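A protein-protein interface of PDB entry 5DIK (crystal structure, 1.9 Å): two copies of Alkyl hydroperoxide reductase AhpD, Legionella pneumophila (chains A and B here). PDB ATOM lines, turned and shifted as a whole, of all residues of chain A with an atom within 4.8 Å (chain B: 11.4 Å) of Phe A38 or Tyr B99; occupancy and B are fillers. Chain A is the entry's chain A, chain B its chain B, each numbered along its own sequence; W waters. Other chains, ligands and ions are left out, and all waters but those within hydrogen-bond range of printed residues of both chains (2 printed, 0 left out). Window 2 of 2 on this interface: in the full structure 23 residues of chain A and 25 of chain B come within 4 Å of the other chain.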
ATOM      1  N   LEU A  34       6.463  14.999  -6.652  1.00  0.00           N
ATOM      2  CA  LEU A  34       5.223  15.776  -6.573  1.00  0.00           C
ATOM      3  C   LEU A  34       4.138  14.909  -5.977  1.00  0.00           C
ATOM      4  O   LEU A  34       3.459  15.314  -5.039  1.00  0.00           O
ATOM      5  CB  LEU A  34       4.840  16.272  -7.966  1.00  0.00           C
ATOM      6  CG  LEU A  34       3.758  17.300  -8.263  1.00  0.00           C
ATOM      7  CD1 LEU A  34       2.379  16.756  -8.028  1.00  0.00           C
ATOM      8  CD2 LEU A  34       3.973  18.609  -7.528  1.00  0.00           C
ATOM      9  N   MET A  35       3.983  13.694  -6.498  1.00  0.00           N
ATOM     10  CA  MET A  35       2.929  12.816  -6.020  1.00  0.00           C
ATOM     11  C   MET A  35       3.132  12.368  -4.566  1.00  0.00           C
ATOM     12  O   MET A  35       2.156  12.216  -3.825  1.00  0.00           O
ATOM     13  CB  MET A  35       2.746  11.608  -6.946  1.00  0.00           C
ATOM     14  CG  MET A  35       2.285  11.985  -8.340  1.00  0.00           C
ATOM     15  SD  MET A  35       0.752  12.943  -8.312  1.00  0.00           S
ATOM     16  CE  MET A  35      -0.396  11.646  -7.905  1.00  0.00           C
ATOM     17  N   THR A  36       4.373  12.128  -4.162  1.00  0.00           N
ATOM     18  CA  THR A  36       4.689  11.829  -2.774  1.00  0.00           C
ATOM     19  C   THR A  36       4.330  12.999  -1.853  1.00  0.00           C
ATOM     20  O   THR A  36       3.734  12.799  -0.805  1.00  0.00           O
ATOM     21  CB  THR A  36       6.181  11.478  -2.601  1.00  0.00           C
ATOM     22  OG1 THR A  36       6.436  10.292  -3.352  1.00  0.00           O
ATOM     23  CG2 THR A  36       6.524  11.238  -1.127  1.00  0.00           C
ATOM     24  N   GLY A  37       4.673  14.208  -2.259  1.00  0.00           N
ATOM     25  CA  GLY A  37       4.288  15.415  -1.501  1.00  0.00           C
ATOM     26  C   GLY A  37       2.781  15.559  -1.378  1.00  0.00           C
ATOM     27  O   GLY A  37       2.254  15.769  -0.298  1.00  0.00           O
ATOM     28  N   PHE A  38       2.079  15.417  -2.504  1.00  0.00           N
ATOM     29  CA  PHE A  38       0.630  15.502  -2.497  1.00  0.00           C
ATOM     30  C   PHE A  38       0.004  14.426  -1.579  1.00  0.00           C
ATOM     31  O   PHE A  38      -0.879  14.736  -0.784  1.00  0.00           O
ATOM     32  CB  PHE A  38       0.039  15.364  -3.891  1.00  0.00           C
ATOM     33  CG  PHE A  38      -1.443  15.537  -3.898  1.00  0.00           C
ATOM     34  CD1 PHE A  38      -1.992  16.804  -3.788  1.00  0.00           C
ATOM     35  CD2 PHE A  38      -2.285  14.445  -3.898  1.00  0.00           C
ATOM     36  CE1 PHE A  38      -3.374  16.969  -3.704  1.00  0.00           C
ATOM     37  CE2 PHE A  38      -3.645  14.607  -3.836  1.00  0.00           C
ATOM     38  CZ  PHE A  38      -4.189  15.859  -3.754  1.00  0.00           C
ATOM     39  N   SER A  39       0.472  13.186  -1.684  1.00  0.00           N
ATOM     40  CA  SER A  39       0.014  12.102  -0.792  1.00  0.00           C
ATOM     41  C   SER A  39       0.251  12.401   0.670  1.00  0.00           C
ATOM     42  O   SER A  39      -0.590  12.075   1.473  1.00  0.00           O
ATOM     43  CB  SER A  39       0.692  10.749  -1.119  1.00  0.00           C
ATOM     44  OG  SER A  39       0.193  10.247  -2.335  1.00  0.00           O
ATOM     45  N   SER A  40       1.409  12.967   1.008  1.00  0.00           N
ATOM     46  CA  SER A  40       1.702  13.347   2.380  1.00  0.00           C
ATOM     47  C   SER A  40       0.719  14.392   2.900  1.00  0.00           C
ATOM     48  O   SER A  40       0.232  14.281   4.026  1.00  0.00           O
ATOM     49  CB  SER A  40       3.133  13.874   2.523  1.00  0.00           C
ATOM     50  OG  SER A  40       4.049  12.841   2.249  1.00  0.00           O
ATOM     51  N   LEU A  41       0.420  15.395   2.076  1.00  0.00           N
ATOM     52  CA  LEU A  41      -0.622  16.361   2.424  1.00  0.00           C
ATOM     53  C   LEU A  41      -1.967  15.667   2.595  1.00  0.00           C
ATOM     54  O   LEU A  41      -2.654  15.898   3.595  1.00  0.00           O
ATOM     55  CB  LEU A  41      -0.721  17.460   1.358  1.00  0.00           C
ATOM     56  CG  LEU A  41      -1.877  18.443   1.486  1.00  0.00           C
ATOM     57  CD1 LEU A  41      -1.713  19.249   2.760  1.00  0.00           C
ATOM     58  CD2 LEU A  41      -1.902  19.387   0.274  1.00  0.00           C
ATOM     59  N   ALA A  42      -2.359  14.819   1.647  1.00  0.00           N
ATOM     60  CA  ALA A  42      -3.662  14.156   1.728  1.00  0.00           C
ATOM     61  C   ALA A  42      -3.799  13.297   2.972  1.00  0.00           C
ATOM     62  O   ALA A  42      -4.851  13.303   3.631  1.00  0.00           O
ATOM     63  CB  ALA A  42      -3.935  13.338   0.475  1.00  0.00           C
ATOM     64  N   ALA A  45      -4.112  15.470   6.079  1.00  0.00           N
ATOM     65  CA  ALA A  45      -5.412  16.114   6.131  1.00  0.00           C
ATOM     66  C   ALA A  45      -6.547  15.185   6.533  1.00  0.00           C
ATOM     67  O   ALA A  45      -7.466  15.614   7.244  1.00  0.00           O
ATOM     68  CB  ALA A  45      -5.735  16.764   4.793  1.00  0.00           C
ATOM     69  N   THR A  46      -6.514  13.939   6.061  1.00  0.00           N
ATOM     70  CA  THR A  46      -7.633  12.997   6.228  1.00  0.00           C
ATOM     71  C   THR A  46      -7.502  12.013   7.392  1.00  0.00           C
ATOM     72  O   THR A  46      -8.429  11.257   7.646  1.00  0.00           O
ATOM     73  CB  THR A  46      -7.827  12.141   4.967  1.00  0.00           C
ATOM     74  OG1 THR A  46      -6.587  11.483   4.684  1.00  0.00           O
ATOM     75  CG2 THR A  46      -8.240  13.013   3.786  1.00  0.00           C
ATOM     76  N   HIS A  76     -14.563  10.938  -3.870  1.00  0.00           N
ATOM     77  CA  HIS A  76     -15.032  11.091  -2.505  1.00  0.00           C
ATOM     78  C   HIS A  76     -16.326  10.311  -2.217  1.00  0.00           C
ATOM     79  O   HIS A  76     -16.504   9.845  -1.094  1.00  0.00           O
ATOM     80  CB  HIS A  76     -15.127  12.573  -2.122  1.00  0.00           C
ATOM     81  CG  HIS A  76     -13.786  13.233  -2.123  1.00  0.00           C
ATOM     82  ND1 HIS A  76     -12.741  12.780  -1.341  1.00  0.00           N
ATOM     83  CD2 HIS A  76     -13.283  14.229  -2.877  1.00  0.00           C
ATOM     84  CE1 HIS A  76     -11.660  13.497  -1.584  1.00  0.00           C
ATOM     85  NE2 HIS A  76     -11.963  14.397  -2.500  1.00  0.00           N
ATOM     86  N   ALA B  62     -15.298  25.199   6.131  1.00  0.00           N
ATOM     87  CA  ALA B  62     -14.502  24.697   5.024  1.00  0.00           C
ATOM     88  C   ALA B  62     -14.887  25.314   3.676  1.00  0.00           C
ATOM     89  O   ALA B  62     -14.007  25.677   2.903  1.00  0.00           O
ATOM     90  CB  ALA B  62     -14.587  23.185   4.927  1.00  0.00           C
ATOM     91  N   LEU B  63     -16.199  25.374   3.402  1.00  0.00           N
ATOM     92  CA  LEU B  63     -16.730  25.975   2.185  1.00  0.00           C
ATOM     93  C   LEU B  63     -16.404  27.475   2.108  1.00  0.00           C
ATOM     94  O   LEU B  63     -16.078  27.987   1.047  1.00  0.00           O
ATOM     95  CB  LEU B  63     -18.251  25.805   2.137  1.00  0.00           C
ATOM     96  CG  LEU B  63     -18.724  24.388   1.869  1.00  0.00           C
ATOM     97  CD1 LEU B  63     -20.190  24.198   2.233  1.00  0.00           C
ATOM     98  CD2 LEU B  63     -18.549  24.079   0.411  1.00  0.00           C
ATOM     99  N   VAL B  65     -13.755  28.990   3.392  1.00  0.00           N
ATOM    100  CA  VAL B  65     -12.354  29.044   3.086  1.00  0.00           C
ATOM    101  C   VAL B  65     -12.133  28.721   1.601  1.00  0.00           C
ATOM    102  O   VAL B  65     -11.448  29.472   0.896  1.00  0.00           O
ATOM    103  CB  VAL B  65     -11.554  28.104   4.005  1.00  0.00           C
ATOM    104  CG1 VAL B  65     -10.135  27.879   3.501  1.00  0.00           C
ATOM    105  CG2 VAL B  65     -11.561  28.671   5.417  1.00  0.00           C
ATOM    106  N   ALA B  66     -12.755  27.631   1.129  1.00  0.00           N
ATOM    107  CA  ALA B  66     -12.682  27.277  -0.284  1.00  0.00           C
ATOM    108  C   ALA B  66     -13.228  28.376  -1.205  1.00  0.00           C
ATOM    109  O   ALA B  66     -12.683  28.597  -2.253  1.00  0.00           O
ATOM    110  CB  ALA B  66     -13.402  25.950  -0.583  1.00  0.00           C
ATOM    111  N   LEU B  90     -11.599  22.993  14.439  1.00  0.00           N
ATOM    112  CA  LEU B  90     -11.390  23.986  13.391  1.00  0.00           C
ATOM    113  C   LEU B  90     -10.140  23.685  12.558  1.00  0.00           C
ATOM    114  O   LEU B  90     -10.212  23.662  11.323  1.00  0.00           O
ATOM    115  CB  LEU B  90     -11.274  25.388  13.994  1.00  0.00           C
ATOM    116  CG  LEU B  90     -10.855  26.481  13.036  1.00  0.00           C
ATOM    117  CD1 LEU B  90     -11.977  26.698  12.035  1.00  0.00           C
ATOM    118  CD2 LEU B  90     -10.525  27.789  13.730  1.00  0.00           C
ATOM    119  N   LEU B  91      -9.004  23.426  13.220  1.00  0.00           N
ATOM    120  CA  LEU B  91      -7.772  23.134  12.513  1.00  0.00           C
ATOM    121  C   LEU B  91      -7.934  21.952  11.578  1.00  0.00           C
ATOM    122  O   LEU B  91      -7.420  21.968  10.476  1.00  0.00           O
ATOM    123  CB  LEU B  91      -6.622  22.859  13.479  1.00  0.00           C
ATOM    124  CG  LEU B  91      -6.144  24.067  14.306  1.00  0.00           C
ATOM    125  CD1 LEU B  91      -5.087  23.609  15.291  1.00  0.00           C
ATOM    126  CD2 LEU B  91      -5.613  25.181  13.423  1.00  0.00           C
ATOM    127  N   GLU B  92      -8.616  20.903  12.030  1.00  0.00           N
ATOM    128  CA  GLU B  92      -8.782  19.712  11.187  1.00  0.00           C
ATOM    129  C   GLU B  92      -9.664  19.991   9.958  1.00  0.00           C
ATOM    130  O   GLU B  92      -9.419  19.467   8.870  1.00  0.00           O
ATOM    131  CB  GLU B  92      -9.294  18.536  12.011  1.00  0.00           C
ATOM    132  CG  GLU B  92      -8.219  18.083  13.001  1.00  0.00           C
ATOM    133  CD  GLU B  92      -8.576  16.845  13.788  1.00  0.00           C
ATOM    134  OE1 GLU B  92      -9.487  16.097  13.337  1.00  0.00           O
ATOM    135  OE2 GLU B  92      -7.947  16.619  14.867  1.00  0.00           O
ATOM    136  N   THR B  93     -10.673  20.832  10.135  1.00  0.00           N
ATOM    137  CA  THR B  93     -11.498  21.276   9.031  1.00  0.00           C
ATOM    138  C   THR B  93     -10.691  22.124   8.039  1.00  0.00           C
ATOM    139  O   THR B  93     -10.810  21.954   6.823  1.00  0.00           O
ATOM    140  CB  THR B  93     -12.728  22.046   9.535  1.00  0.00           C
ATOM    141  OG1 THR B  93     -13.406  21.231  10.510  1.00  0.00           O
ATOM    142  CG2 THR B  93     -13.646  22.301   8.419  1.00  0.00           C
ATOM    143  N   LEU B  94      -9.860  23.034   8.558  1.00  0.00           N
ATOM    144  CA  LEU B  94      -8.993  23.831   7.687  1.00  0.00           C
ATOM    145  C   LEU B  94      -7.994  22.976   6.914  1.00  0.00           C
ATOM    146  O   LEU B  94      -7.711  23.247   5.735  1.00  0.00           O
ATOM    147  CB  LEU B  94      -8.273  24.918   8.493  1.00  0.00           C
ATOM    148  CG  LEU B  94      -9.245  25.919   9.165  1.00  0.00           C
ATOM    149  CD1 LEU B  94      -8.490  26.940  10.019  1.00  0.00           C
ATOM    150  CD2 LEU B  94     -10.106  26.632   8.142  1.00  0.00           C
ATOM    151  N   GLY B  95      -7.497  21.917   7.535  1.00  0.00           N
ATOM    152  CA  GLY B  95      -6.625  20.991   6.851  1.00  0.00           C
ATOM    153  C   GLY B  95      -7.265  20.369   5.618  1.00  0.00           C
ATOM    154  O   GLY B  95      -6.630  20.193   4.576  1.00  0.00           O
ATOM    155  N   MET B  96      -8.540  20.022   5.735  1.00  0.00           N
ATOM    156  CA  MET B  96      -9.275  19.462   4.594  1.00  0.00           C
ATOM    157  C   MET B  96      -9.431  20.497   3.473  1.00  0.00           C
ATOM    158  O   MET B  96      -9.273  20.175   2.313  1.00  0.00           O
ATOM    159  CB  MET B  96     -10.639  18.955   5.033  1.00  0.00           C
ATOM    160  CG  MET B  96     -10.576  17.665   5.852  1.00  0.00           C
ATOM    161  SD  MET B  96      -9.755  16.318   4.986  1.00  0.00           S
ATOM    162  CE  MET B  96     -10.777  16.088   3.541  1.00  0.00           C
ATOM    163  N   ALA B  97      -9.675  21.752   3.837  1.00  0.00           N
ATOM    164  CA  ALA B  97      -9.727  22.824   2.873  1.00  0.00           C
ATOM    165  C   ALA B  97      -8.392  22.974   2.129  1.00  0.00           C
ATOM    166  O   ALA B  97      -8.384  23.179   0.909  1.00  0.00           O
ATOM    167  CB  ALA B  97     -10.106  24.151   3.538  1.00  0.00           C
ATOM    168  N   VAL B  98      -7.273  22.865   2.828  1.00  0.00           N
ATOM    169  CA  VAL B  98      -5.960  22.991   2.190  1.00  0.00           C
ATOM    170  C   VAL B  98      -5.687  21.827   1.225  1.00  0.00           C
ATOM    171  O   VAL B  98      -5.210  22.009   0.108  1.00  0.00           O
ATOM    172  CB  VAL B  98      -4.829  23.129   3.223  1.00  0.00           C
ATOM    173  CG1 VAL B  98      -3.475  23.117   2.528  1.00  0.00           C
ATOM    174  CG2 VAL B  98      -5.003  24.429   3.994  1.00  0.00           C
ATOM    175  N   TYR B  99      -6.017  20.627   1.648  1.00  0.00           N
ATOM    176  CA  TYR B  99      -5.930  19.481   0.790  1.00  0.00           C
ATOM    177  C   TYR B  99      -6.739  19.671  -0.515  1.00  0.00           C
ATOM    178  O   TYR B  99      -6.264  19.307  -1.597  1.00  0.00           O
ATOM    179  CB  TYR B  99      -6.366  18.234   1.578  1.00  0.00           C
ATOM    180  CG  TYR B  99      -6.874  17.062   0.768  1.00  0.00           C
ATOM    181  CD1 TYR B  99      -6.125  16.516  -0.263  1.00  0.00           C
ATOM    182  CD2 TYR B  99      -8.057  16.423   1.124  1.00  0.00           C
ATOM    183  CE1 TYR B  99      -6.580  15.409  -0.979  1.00  0.00           C
ATOM    184  CE2 TYR B  99      -8.524  15.317   0.431  1.00  0.00           C
ATOM    185  CZ  TYR B  99      -7.784  14.813  -0.617  1.00  0.00           C
ATOM    186  OH  TYR B  99      -8.270  13.735  -1.305  1.00  0.00           O
ATOM    187  N   MET B 100      -7.930  20.275  -0.426  1.00  0.00           N
ATOM    188  CA  MET B 100      -8.811  20.449  -1.576  1.00  0.00           C
ATOM    189  C   MET B 100      -8.642  21.813  -2.265  1.00  0.00           C
ATOM    190  O   MET B 100      -9.404  22.150  -3.144  1.00  0.00           O
ATOM    191  CB  MET B 100     -10.280  20.328  -1.134  1.00  0.00           C
ATOM    192  CG  MET B 100     -10.607  18.965  -0.535  1.00  0.00           C
ATOM    193  SD  MET B 100     -10.682  17.843  -1.902  1.00  0.00           S
ATOM    194  CE  MET B 100     -12.206  18.216  -2.791  1.00  0.00           C
ATOM    195  N   GLY B 101      -7.670  22.607  -1.859  1.00  0.00           N
ATOM    196  CA  GLY B 101      -7.540  23.928  -2.423  1.00  0.00           C
ATOM    197  C   GLY B 101      -6.113  24.419  -2.618  1.00  0.00           C
ATOM    198  O   GLY B 101      -5.907  25.423  -3.298  1.00  0.00           O
ATOM    199  N   GLY B 102      -5.128  23.753  -2.011  1.00  0.00           N
ATOM    200  CA  GLY B 102      -3.751  24.181  -2.145  1.00  0.00           C
ATOM    201  C   GLY B 102      -3.449  25.554  -1.556  1.00  0.00           C
ATOM    202  O   GLY B 102      -4.074  25.990  -0.570  1.00  0.00           O
ATOM    203  N   GLY B 103      -2.443  26.203  -2.136  1.00  0.00           N
ATOM    204  CA  GLY B 103      -1.884  27.459  -1.602  1.00  0.00           C
ATOM    205  C   GLY B 103      -2.924  28.485  -1.238  1.00  0.00           C
ATOM    206  O   GLY B 103      -2.907  29.038  -0.117  1.00  0.00           O
ATOM    207  N   PRO B 104      -3.842  28.776  -2.159  1.00  0.00           N
ATOM    208  CA  PRO B 104      -4.854  29.778  -1.850  1.00  0.00           C
ATOM    209  C   PRO B 104      -5.679  29.463  -0.616  1.00  0.00           C
ATOM    210  O   PRO B 104      -6.008  30.378   0.191  1.00  0.00           O
ATOM    211  CB  PRO B 104      -5.709  29.803  -3.129  1.00  0.00           C
ATOM    212  CG  PRO B 104      -4.729  29.476  -4.192  1.00  0.00           C
ATOM    213  CD  PRO B 104      -3.842  28.438  -3.597  1.00  0.00           C
ATOM    214  N   SER B 105      -6.044  28.190  -0.453  1.00  0.00           N
ATOM    215  CA  SER B 105      -6.809  27.814   0.710  1.00  0.00           C
ATOM    216  C   SER B 105      -6.011  27.926   1.976  1.00  0.00           C
ATOM    217  O   SER B 105      -6.573  28.167   3.007  1.00  0.00           O
ATOM    218  CB  SER B 105      -7.428  26.427   0.553  1.00  0.00           C
ATOM    219  OG  SER B 105      -8.437  26.478  -0.455  1.00  0.00           O
ATOM    220  N   LEU B 106      -4.709  27.686   1.900  1.00  0.00           N
ATOM    221  CA  LEU B 106      -3.836  27.899   3.056  1.00  0.00           C
ATOM    222  C   LEU B 106      -3.893  29.362   3.485  1.00  0.00           C
ATOM    223  O   LEU B 106      -3.949  29.641   4.682  1.00  0.00           O
ATOM    224  CB  LEU B 106      -2.416  27.464   2.739  1.00  0.00           C
ATOM    225  CG  LEU B 106      -1.443  27.529   3.904  1.00  0.00           C
ATOM    226  CD1 LEU B 106      -1.893  26.606   5.014  1.00  0.00           C
ATOM    227  CD2 LEU B 106      -0.054  27.196   3.397  1.00  0.00           C
ATOM    228  N   MET B 107      -3.958  30.283   2.525  1.00  0.00           N
ATOM    229  CA  MET B 107      -4.058  31.737   2.839  1.00  0.00           C
ATOM    230  C   MET B 107      -5.369  32.082   3.573  1.00  0.00           C
ATOM    231  O   MET B 107      -5.364  32.844   4.553  1.00  0.00           O
ATOM    232  CB  MET B 107      -3.985  32.575   1.570  1.00  0.00           C
ATOM    233  CG  MET B 107      -2.761  32.361   0.705  1.00  0.00           C
ATOM    234  SD  MET B 107      -1.180  32.780   1.515  1.00  0.00           S
ATOM    235  CE  MET B 107      -0.647  31.216   2.156  1.00  0.00           C
ATOM    236  N   TYR B 108      -6.498  31.502   3.131  1.00  0.00           N
ATOM    237  CA  TYR B 108      -7.764  31.742   3.796  1.00  0.00           C
ATOM    238  C   TYR B 108      -7.928  30.916   5.064  1.00  0.00           C
ATOM    239  O   TYR B 108      -8.668  31.322   5.976  1.00  0.00           O
ATOM    240  CB  TYR B 108      -8.934  31.567   2.817  1.00  0.00           C
ATOM    241  CG  TYR B 108      -8.957  32.738   1.886  1.00  0.00           C
ATOM    242  CD1 TYR B 108      -9.550  33.942   2.267  1.00  0.00           C
ATOM    243  CD2 TYR B 108      -8.292  32.697   0.667  1.00  0.00           C
ATOM    244  CE1 TYR B 108      -9.530  35.036   1.421  1.00  0.00           C
ATOM    245  CE2 TYR B 108      -8.229  33.811  -0.159  1.00  0.00           C
ATOM    246  CZ  TYR B 108      -8.845  34.971   0.233  1.00  0.00           C
ATOM    247  OH  TYR B 108      -8.811  36.057  -0.633  1.00  0.00           O
ATOM    248  N   ALA B 109      -7.227  29.783   5.168  1.00  0.00           N
ATOM    249  CA  ALA B 109      -7.192  29.080   6.453  1.00  0.00           C
ATOM    250  C   ALA B 109      -6.547  29.983   7.545  1.00  0.00           C
ATOM    251  O   ALA B 109      -7.000  30.007   8.685  1.00  0.00           O
ATOM    252  CB  ALA B 109      -6.439  27.782   6.352  1.00  0.00           C
HETATM  253  O   HOH W   1     -10.048  15.881  -4.403  1.00  0.00           O
HETATM  254  O   HOH W   2      -7.336  17.985   8.507  1.00  0.00           O
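Printed residues of chain A that touch a printed residue of chain B: Phe A38, Ala A42, Ala A45, Thr A46 and His A76. Of the 24 printed residues of chain B, 4 touch a printed residue of chain A. Among the printed residues, no Asp or Glu carboxylate lies within 4 Å of a Lys or Arg side-chain nitrogen of the other chain.
Phe A38 touches one residue of chain B. Tyr B99 touches four residues of chain A. No residue of chain B comes within 4 Å of Leu A34. No residue of chain B comes within 4 Å of Met A35. No residue of chain B comes within 4 Å of Thr A36. No residue of chain B comes within 4 Å of Gly A37. No residue of chain B comes within 4 Å of Ser A39. Leu A41 touches none of the printed residues of chain B. Ala A42 touches just one residue of chain B: Tyr B99 (3.7 Å). Of the printed residues of chain A, Gly B95 touches Ala A45 (3.6 Å). Of the printed residues of chain B, Thr A46 touches Met B96. Printed residues of chain A within 4 Å of Met B96: Ala A45 (3.3 Å) and Thr A46 (3.8 Å). Gly B101 touches none of the printed residues of chain A. Val B65 touches none of the printed residues of chain A. The nearest printed residue of chain A that does not touch Tyr B99 is Leu A41 (4.1 Å). The nearest printed residue of chain B that does not touch His A76 is Met B96 (5.8 Å).
A ring nitrogen (NE2) of His A76 sits at hydrogen-bond distance from the side-chain sulfur of Met B100 (3.7 Å). The backbone carbonyl oxygen (O) of Ala A45 sits close to the side-chain sulfur (SD) of Met B96 (3.3 Å).
Water W2 bridges O of Glu B92 (2.6 Å) and O of Ala A45 (2.7 Å). Water W1 bridges a ring nitrogen (NE2) of His A76 (3.1 Å) and the side-chain sulfur (SD) of Met B100 (3.2 Å).
No position is printed for both chains. Of the 8 pairs that touch across the chains among the printed residues, none has its exchanged pair printed and touching as well.
The backbone carbonyl oxygen of Ala A42 is in hydrogen-bond range of the side-chain hydroxyl of Thr A46 (2.7 Å).
Tyr B99 touches Phe A38. CB of Ala A42 touches CE1 of Tyr B99, at 3.7 Å. CB of Ala A45 touches O of Gly B95, at 3.6 Å. CB of Ala A45 touches CB of Tyr B99, at 3.6 Å. Met B96 touches Thr A46. OH of Tyr B99 touches CE1 of His A76 (3.4 Å).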
